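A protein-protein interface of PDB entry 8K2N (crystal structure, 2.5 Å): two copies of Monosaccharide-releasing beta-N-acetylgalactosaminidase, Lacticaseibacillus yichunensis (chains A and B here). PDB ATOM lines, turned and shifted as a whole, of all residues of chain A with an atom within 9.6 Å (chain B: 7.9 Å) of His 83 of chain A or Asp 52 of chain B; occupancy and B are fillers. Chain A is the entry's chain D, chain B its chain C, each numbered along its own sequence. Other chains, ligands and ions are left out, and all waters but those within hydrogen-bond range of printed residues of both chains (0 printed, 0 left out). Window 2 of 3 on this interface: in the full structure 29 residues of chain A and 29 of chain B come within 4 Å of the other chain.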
ATOM      1  N   LEU A  78      24.614  -8.328 -24.108  1.00  0.00           N
ATOM      2  CA  LEU A  78      24.844  -9.708 -24.507  1.00  0.00           C
ATOM      3  C   LEU A  78      25.638  -9.691 -25.808  1.00  0.00           C
ATOM      4  O   LEU A  78      25.109  -9.842 -26.908  1.00  0.00           O
ATOM      5  CB  LEU A  78      23.513 -10.441 -24.683  1.00  0.00           C
ATOM      6  CG  LEU A  78      23.602 -11.953 -24.920  1.00  0.00           C
ATOM      7  CD1 LEU A  78      24.081 -12.648 -23.661  1.00  0.00           C
ATOM      8  CD2 LEU A  78      22.264 -12.554 -25.328  1.00  0.00           C
ATOM      9  N   THR A  80      27.797 -11.782 -27.025  1.00  0.00           N
ATOM     10  CA  THR A  80      27.955 -13.114 -27.617  1.00  0.00           C
ATOM     11  C   THR A  80      27.015 -14.145 -26.992  1.00  0.00           C
ATOM     12  O   THR A  80      26.527 -13.976 -25.882  1.00  0.00           O
ATOM     13  CB  THR A  80      29.379 -13.707 -27.517  1.00  0.00           C
ATOM     14  OG1 THR A  80      29.540 -14.387 -26.272  1.00  0.00           O
ATOM     15  CG2 THR A  80      30.482 -12.678 -27.719  1.00  0.00           C
ATOM     16  N   TRP A  81      26.745 -15.212 -27.774  1.00  0.00           N
ATOM     17  CA  TRP A  81      26.082 -16.430 -27.315  1.00  0.00           C
ATOM     18  C   TRP A  81      27.171 -17.303 -26.691  1.00  0.00           C
ATOM     19  O   TRP A  81      28.340 -16.936 -26.751  1.00  0.00           O
ATOM     20  CB  TRP A  81      25.363 -17.122 -28.506  1.00  0.00           C
ATOM     21  CG  TRP A  81      23.894 -16.802 -28.603  1.00  0.00           C
ATOM     22  CD1 TRP A  81      23.236 -15.816 -27.925  1.00  0.00           C
ATOM     23  CD2 TRP A  81      22.885 -17.544 -29.306  1.00  0.00           C
ATOM     24  NE1 TRP A  81      21.903 -15.861 -28.185  1.00  0.00           N
ATOM     25  CE2 TRP A  81      21.646 -16.900 -29.044  1.00  0.00           C
ATOM     26  CE3 TRP A  81      22.899 -18.692 -30.121  1.00  0.00           C
ATOM     27  CZ2 TRP A  81      20.416 -17.348 -29.576  1.00  0.00           C
ATOM     28  CZ3 TRP A  81      21.693 -19.109 -30.694  1.00  0.00           C
ATOM     29  CH2 TRP A  81      20.468 -18.451 -30.410  1.00  0.00           C
ATOM     30  N   PRO A  82      26.851 -18.436 -26.025  1.00  0.00           N
ATOM     31  CA  PRO A  82      27.884 -19.248 -25.358  1.00  0.00           C
ATOM     32  C   PRO A  82      29.001 -19.811 -26.239  1.00  0.00           C
ATOM     33  O   PRO A  82      28.769 -20.103 -27.387  1.00  0.00           O
ATOM     34  CB  PRO A  82      27.010 -20.361 -24.779  1.00  0.00           C
ATOM     35  CG  PRO A  82      25.706 -19.651 -24.442  1.00  0.00           C
ATOM     36  CD  PRO A  82      25.478 -18.850 -25.699  1.00  0.00           C
ATOM     37  N   HIS A  83      30.211 -19.961 -25.683  1.00  0.00           N
ATOM     38  CA  HIS A  83      31.365 -20.633 -26.267  1.00  0.00           C
ATOM     39  C   HIS A  83      31.872 -19.787 -27.420  1.00  0.00           C
ATOM     40  O   HIS A  83      32.180 -20.329 -28.467  1.00  0.00           O
ATOM     41  CB  HIS A  83      31.116 -22.116 -26.692  1.00  0.00           C
ATOM     42  CG  HIS A  83      30.438 -23.006 -25.672  1.00  0.00           C
ATOM     43  ND1 HIS A  83      30.957 -23.253 -24.418  1.00  0.00           N
ATOM     44  CD2 HIS A  83      29.176 -23.526 -25.652  1.00  0.00           C
ATOM     45  CE1 HIS A  83      30.048 -23.886 -23.670  1.00  0.00           C
ATOM     46  NE2 HIS A  83      28.950 -24.075 -24.416  1.00  0.00           N
ATOM     47  N   PRO A  84      32.114 -18.463 -27.274  1.00  0.00           N
ATOM     48  CA  PRO A  84      32.646 -17.659 -28.390  1.00  0.00           C
ATOM     49  C   PRO A  84      34.047 -18.054 -28.854  1.00  0.00           C
ATOM     50  O   PRO A  84      34.917 -18.328 -28.046  1.00  0.00           O
ATOM     51  CB  PRO A  84      32.738 -16.234 -27.812  1.00  0.00           C
ATOM     52  CG  PRO A  84      32.828 -16.433 -26.309  1.00  0.00           C
ATOM     53  CD  PRO A  84      31.995 -17.675 -26.035  1.00  0.00           C
ATOM     54  N   ASP A  85      34.299 -17.998 -30.151  1.00  0.00           N
ATOM     55  CA  ASP A  85      35.561 -18.463 -30.679  1.00  0.00           C
ATOM     56  C   ASP A  85      36.523 -17.274 -30.657  1.00  0.00           C
ATOM     57  O   ASP A  85      36.164 -16.184 -30.198  1.00  0.00           O
ATOM     58  CB  ASP A  85      35.337 -19.139 -32.039  1.00  0.00           C
ATOM     59  CG  ASP A  85      34.917 -18.223 -33.178  1.00  0.00           C
ATOM     60  OD1 ASP A  85      35.381 -17.083 -33.217  1.00  0.00           O
ATOM     61  OD2 ASP A  85      34.203 -18.693 -34.078  1.00  0.00           O
ATOM     62  N   ALA A  86      37.709 -17.455 -31.239  1.00  0.00           N
ATOM     63  CA  ALA A  86      38.810 -16.512 -31.049  1.00  0.00           C
ATOM     64  C   ALA A  86      38.724 -15.296 -31.985  1.00  0.00           C
ATOM     65  O   ALA A  86      39.567 -14.425 -31.842  1.00  0.00           O
ATOM     66  CB  ALA A  86      40.124 -17.222 -31.242  1.00  0.00           C
ATOM     67  N   ARG A  87      37.756 -15.227 -32.922  1.00  0.00           N
ATOM     68  CA  ARG A  87      37.455 -14.013 -33.708  1.00  0.00           C
ATOM     69  C   ARG A  87      36.875 -12.828 -32.873  1.00  0.00           C
ATOM     70  O   ARG A  87      37.061 -11.664 -33.218  1.00  0.00           O
ATOM     71  CB  ARG A  87      36.418 -14.327 -34.814  1.00  0.00           C
ATOM     72  CG  ARG A  87      36.860 -15.342 -35.876  1.00  0.00           C
ATOM     73  CD  ARG A  87      35.708 -15.685 -36.825  1.00  0.00           C
ATOM     74  NE  ARG A  87      34.515 -16.160 -36.140  1.00  0.00           N
ATOM     75  CZ  ARG A  87      33.261 -16.087 -36.615  1.00  0.00           C
ATOM     76  NH1 ARG A  87      32.977 -15.544 -37.794  1.00  0.00           N
ATOM     77  NH2 ARG A  87      32.271 -16.565 -35.868  1.00  0.00           N
ATOM     78  N   TYR A  88      36.101 -13.111 -31.817  1.00  0.00           N
ATOM     79  CA  TYR A  88      35.354 -12.107 -31.096  1.00  0.00           C
ATOM     80  C   TYR A  88      36.317 -11.152 -30.393  1.00  0.00           C
ATOM     81  O   TYR A  88      37.210 -11.611 -29.706  1.00  0.00           O
ATOM     82  CB  TYR A  88      34.385 -12.777 -30.121  1.00  0.00           C
ATOM     83  CG  TYR A  88      33.180 -13.433 -30.740  1.00  0.00           C
ATOM     84  CD1 TYR A  88      33.261 -14.684 -31.379  1.00  0.00           C
ATOM     85  CD2 TYR A  88      31.933 -12.832 -30.651  1.00  0.00           C
ATOM     86  CE1 TYR A  88      32.155 -15.300 -31.960  1.00  0.00           C
ATOM     87  CE2 TYR A  88      30.796 -13.433 -31.210  1.00  0.00           C
ATOM     88  CZ  TYR A  88      30.917 -14.664 -31.877  1.00  0.00           C
ATOM     89  OH  TYR A  88      29.778 -15.217 -32.415  1.00  0.00           O
ATOM     90  N   THR A  91      33.625  -9.652 -25.045  1.00  0.00           N
ATOM     91  CA  THR A  91      32.894 -10.810 -24.587  1.00  0.00           C
ATOM     92  C   THR A  91      31.948 -10.429 -23.474  1.00  0.00           C
ATOM     93  O   THR A  91      30.927 -11.093 -23.364  1.00  0.00           O
ATOM     94  CB  THR A  91      33.877 -11.908 -24.123  1.00  0.00           C
ATOM     95  OG1 THR A  91      33.651 -12.922 -25.114  1.00  0.00           O
ATOM     96  CG2 THR A  91      33.659 -12.431 -22.714  1.00  0.00           C
ATOM     97  N   CYS A 398      21.099 -15.064 -35.323  1.00  0.00           N
ATOM     98  CA  CYS A 398      21.627 -15.245 -33.980  1.00  0.00           C
ATOM     99  C   CYS A 398      22.459 -16.519 -33.874  1.00  0.00           C
ATOM    100  O   CYS A 398      23.396 -16.538 -33.063  1.00  0.00           O
ATOM    101  CB  CYS A 398      20.538 -15.164 -32.902  1.00  0.00           C
ATOM    102  SG  CYS A 398      19.019 -16.141 -33.133  1.00  0.00           S
ATOM    103  N   THR A 401      27.221 -18.603 -35.087  1.00  0.00           N
ATOM    104  CA  THR A 401      28.078 -18.049 -34.040  1.00  0.00           C
ATOM    105  C   THR A 401      29.568 -18.404 -34.236  1.00  0.00           C
ATOM    106  O   THR A 401      30.424 -17.611 -33.788  1.00  0.00           O
ATOM    107  CB  THR A 401      27.572 -18.476 -32.657  1.00  0.00           C
ATOM    108  OG1 THR A 401      27.682 -19.886 -32.708  1.00  0.00           O
ATOM    109  CG2 THR A 401      26.154 -18.076 -32.309  1.00  0.00           C
ATOM    110  N   THR A 402      29.854 -19.444 -35.068  1.00  0.00           N
ATOM    111  CA  THR A 402      31.154 -20.108 -35.149  1.00  0.00           C
ATOM    112  C   THR A 402      31.650 -20.190 -36.599  1.00  0.00           C
ATOM    113  O   THR A 402      31.026 -20.822 -37.450  1.00  0.00           O
ATOM    114  CB  THR A 402      31.064 -21.525 -34.541  1.00  0.00           C
ATOM    115  OG1 THR A 402      30.288 -21.412 -33.352  1.00  0.00           O
ATOM    116  CG2 THR A 402      32.390 -22.158 -34.158  1.00  0.00           C
ATOM    117  N   ALA A 403      32.801 -19.553 -36.876  1.00  0.00           N
ATOM    118  CA  ALA A 403      33.625 -19.787 -38.070  1.00  0.00           C
ATOM    119  C   ALA A 403      33.087 -19.080 -39.306  1.00  0.00           C
ATOM    120  O   ALA A 403      33.777 -19.026 -40.297  1.00  0.00           O
ATOM    121  CB  ALA A 403      33.727 -21.290 -38.360  1.00  0.00           C
ATOM    122  N   ALA A 459      18.507 -11.646 -25.328  1.00  0.00           N
ATOM    123  CA  ALA A 459      18.215 -12.934 -25.950  1.00  0.00           C
ATOM    124  C   ALA A 459      19.190 -13.172 -27.108  1.00  0.00           C
ATOM    125  O   ALA A 459      19.594 -14.306 -27.295  1.00  0.00           O
ATOM    126  CB  ALA A 459      16.767 -12.987 -26.396  1.00  0.00           C
ATOM    127  N   ARG B  47      25.620 -17.342 -13.207  1.00  0.00           N
ATOM    128  CA  ARG B  47      25.687 -18.789 -13.410  1.00  0.00           C
ATOM    129  C   ARG B  47      27.089 -19.156 -13.863  1.00  0.00           C
ATOM    130  O   ARG B  47      27.562 -18.623 -14.862  1.00  0.00           O
ATOM    131  CB  ARG B  47      24.599 -19.289 -14.370  1.00  0.00           C
ATOM    132  CG  ARG B  47      25.052 -20.450 -15.260  1.00  0.00           C
ATOM    133  CD  ARG B  47      24.010 -21.465 -15.650  1.00  0.00           C
ATOM    134  NE  ARG B  47      23.278 -21.187 -16.881  1.00  0.00           N
ATOM    135  CZ  ARG B  47      23.794 -21.069 -18.110  1.00  0.00           C
ATOM    136  NH1 ARG B  47      25.086 -21.156 -18.342  1.00  0.00           N
ATOM    137  NH2 ARG B  47      22.979 -20.810 -19.114  1.00  0.00           N
ATOM    138  N   ARG B  49      28.082 -22.525 -14.529  1.00  0.00           N
ATOM    139  CA  ARG B  49      27.913 -23.622 -15.483  1.00  0.00           C
ATOM    140  C   ARG B  49      27.843 -23.027 -16.889  1.00  0.00           C
ATOM    141  O   ARG B  49      26.979 -22.149 -17.164  1.00  0.00           O
ATOM    142  CB  ARG B  49      26.654 -24.416 -15.085  1.00  0.00           C
ATOM    143  CG  ARG B  49      26.107 -25.444 -16.068  1.00  0.00           C
ATOM    144  CD  ARG B  49      24.812 -26.107 -15.528  1.00  0.00           C
ATOM    145  NE  ARG B  49      23.494 -25.482 -15.774  1.00  0.00           N
ATOM    146  CZ  ARG B  49      22.516 -25.344 -14.867  1.00  0.00           C
ATOM    147  NH1 ARG B  49      22.644 -25.761 -13.612  1.00  0.00           N
ATOM    148  NH2 ARG B  49      21.383 -24.758 -15.204  1.00  0.00           N
ATOM    149  N   ASP B  50      28.774 -23.526 -17.734  1.00  0.00           N
ATOM    150  CA  ASP B  50      28.970 -23.082 -19.109  1.00  0.00           C
ATOM    151  C   ASP B  50      28.216 -23.954 -20.134  1.00  0.00           C
ATOM    152  O   ASP B  50      28.831 -24.457 -21.082  1.00  0.00           O
ATOM    153  CB  ASP B  50      30.461 -23.024 -19.427  1.00  0.00           C
ATOM    154  CG  ASP B  50      30.774 -22.216 -20.674  1.00  0.00           C
ATOM    155  OD1 ASP B  50      29.813 -21.532 -21.229  1.00  0.00           O
ATOM    156  OD2 ASP B  50      31.972 -22.226 -21.081  1.00  0.00           O
ATOM    157  N   ASP B  51      26.870 -24.013 -20.041  1.00  0.00           N
ATOM    158  CA  ASP B  51      26.030 -24.813 -20.936  1.00  0.00           C
ATOM    159  C   ASP B  51      25.796 -24.063 -22.263  1.00  0.00           C
ATOM    160  O   ASP B  51      26.576 -23.196 -22.641  1.00  0.00           O
ATOM    161  CB  ASP B  51      24.794 -25.361 -20.182  1.00  0.00           C
ATOM    162  CG  ASP B  51      23.813 -24.385 -19.509  1.00  0.00           C
ATOM    163  OD1 ASP B  51      22.839 -23.922 -20.164  1.00  0.00           O
ATOM    164  OD2 ASP B  51      23.955 -24.162 -18.288  1.00  0.00           O
ATOM    165  N   ASP B  52      24.740 -24.426 -23.004  1.00  0.00           N
ATOM    166  CA  ASP B  52      24.455 -23.866 -24.323  1.00  0.00           C
ATOM    167  C   ASP B  52      23.379 -22.762 -24.323  1.00  0.00           C
ATOM    168  O   ASP B  52      23.241 -22.064 -25.323  1.00  0.00           O
ATOM    169  CB  ASP B  52      24.057 -25.015 -25.251  1.00  0.00           C
ATOM    170  CG  ASP B  52      25.196 -25.985 -25.523  1.00  0.00           C
ATOM    171  OD1 ASP B  52      26.365 -25.672 -25.254  1.00  0.00           O
ATOM    172  OD2 ASP B  52      24.903 -27.047 -26.001  1.00  0.00           O
ATOM    173  N   ALA B  53      22.586 -22.643 -23.244  1.00  0.00           N
ATOM    174  CA  ALA B  53      21.787 -21.460 -22.929  1.00  0.00           C
ATOM    175  C   ALA B  53      22.648 -20.326 -22.313  1.00  0.00           C
ATOM    176  O   ALA B  53      23.533 -20.551 -21.475  1.00  0.00           O
ATOM    177  CB  ALA B  53      20.688 -21.848 -21.967  1.00  0.00           C
ATOM    178  N   SER B  54      22.356 -19.073 -22.698  1.00  0.00           N
ATOM    179  CA  SER B  54      23.004 -17.880 -22.177  1.00  0.00           C
ATOM    180  C   SER B  54      22.639 -17.678 -20.714  1.00  0.00           C
ATOM    181  O   SER B  54      23.501 -17.325 -19.956  1.00  0.00           O
ATOM    182  CB  SER B  54      22.673 -16.659 -23.026  1.00  0.00           C
ATOM    183  OG  SER B  54      23.278 -16.810 -24.305  1.00  0.00           O
ATOM    184  N   PHE B  55      21.432 -18.050 -20.293  1.00  0.00           N
ATOM    185  CA  PHE B  55      20.985 -17.868 -18.916  1.00  0.00           C
ATOM    186  C   PHE B  55      20.081 -19.009 -18.402  1.00  0.00           C
ATOM    187  O   PHE B  55      19.570 -19.806 -19.165  1.00  0.00           O
ATOM    188  CB  PHE B  55      20.184 -16.563 -18.810  1.00  0.00           C
ATOM    189  CG  PHE B  55      18.993 -16.438 -19.732  1.00  0.00           C
ATOM    190  CD1 PHE B  55      19.114 -15.986 -21.053  1.00  0.00           C
ATOM    191  CD2 PHE B  55      17.715 -16.758 -19.280  1.00  0.00           C
ATOM    192  CE1 PHE B  55      17.987 -15.856 -21.875  1.00  0.00           C
ATOM    193  CE2 PHE B  55      16.610 -16.681 -20.128  1.00  0.00           C
ATOM    194  CZ  PHE B  55      16.732 -16.177 -21.397  1.00  0.00           C
ATOM    195  N   HIS B 111      25.650 -16.622 -17.742  1.00  0.00           N
ATOM    196  CA  HIS B 111      27.056 -16.991 -17.705  1.00  0.00           C
ATOM    197  C   HIS B 111      27.887 -15.846 -18.272  1.00  0.00           C
ATOM    198  O   HIS B 111      27.506 -15.223 -19.256  1.00  0.00           O
ATOM    199  CB  HIS B 111      27.354 -18.292 -18.478  1.00  0.00           C
ATOM    200  CG  HIS B 111      28.826 -18.600 -18.575  1.00  0.00           C
ATOM    201  ND1 HIS B 111      29.646 -18.008 -19.504  1.00  0.00           N
ATOM    202  CD2 HIS B 111      29.632 -19.445 -17.890  1.00  0.00           C
ATOM    203  CE1 HIS B 111      30.913 -18.439 -19.335  1.00  0.00           C
ATOM    204  NE2 HIS B 111      30.923 -19.324 -18.366  1.00  0.00           N
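No position is printed for both chains.
CD1 of Trp 81 of chain A touches OG of Ser 54 of chain B, at 3.8 Å.
Pro 82 of chain A touches Asp 51 of chain B.
Pro 82 of chain A touches Asp 52 of chain B.
Ala 53 of chain B touches Pro 82 of chain A.
CD of Pro 82 of chain A touches OG of Ser 54 of chain B, 3.3 Å away.
Of the 9 printed residues of chain B, 5 touch a printed residue of chain A.
Of the 16 printed residues of chain A, 3 touch a printed residue of chain B.
Printed residues of chain A that touch a printed residue of chain B: Trp 81, Pro 82 and His 83.
Hydrophobic or aromatic side chains of chain A that line the printed part of chain B: Trp 81, Pro 82 and His 83.
Among the printed residues, no Asp or Glu carboxylate lies within 4 Å of a Lys or Arg side-chain nitrogen of the other chain.
NE1 of Trp 81 of chain A sits at hydrogen-bond distance from O of Ala 459 of chain A.
The backbone NH (N) of Ala 53 of chain B lies within hydrogen-bond range of the side-chain carboxylate (OD1) of Asp 51 of chain B, at 3.3 Å.
The guanidinium group (NH2) of Arg 47 of chain B lies within hydrogen-bond range of the backbone carbonyl oxygen (O) of Ala 53 of chain B (2.4 Å).
O of Ser 54 of chain B is in hydrogen-bond range of N of His 111 of chain B, 3.2 Å away.
The guanidinium group (NH1) of Arg 47 of chain B is in salt-bridge range of the side-chain carboxylate (OD2) of Asp 51 of chain B.
NE of Arg 49 of chain B is in salt-bridge range of OD2 of Asp 51 of chain B (2.9 Å).
Of the printed residues of chain B, Trp 81 of chain A touches Ser 54 (3.8 Å).
His 83 of chain A touches just these residues of chain B: Asp 50, Asp 51 and Asp 52.
No residue of chain B comes within 4 Å of Pro 84 of chain A.
Of the printed residues of chain A, Asp 50 of chain B touches His 83 (2.9 Å).
Of chain A, only Pro 82 (3.6 Å) and His 83 (3.1 Å) come within 4 Å of Asp 51 of chain B.
Ala 53 of chain B touches one residue of chain A.
Of the printed residues of chain A, Ser 54 of chain B touches Trp 81 and Pro 82.
The nearest printed residue of chain B that does not touch Pro 82 of chain A is Asp 50 of chain B (4.7 Å).
A ring nitrogen (NE2) of His 83 of chain A lies within hydrogen-bond range of the side-chain carboxylate (OD1) of Asp 52 of chain B (3.2 Å).
NE2 of His 83 of chain A lies within hydrogen-bond range of O of Asp 51 of chain B (3.1 Å).
O of Asp 50 of chain B lies close to NE2 of His 83 of chain A (3.4 Å).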
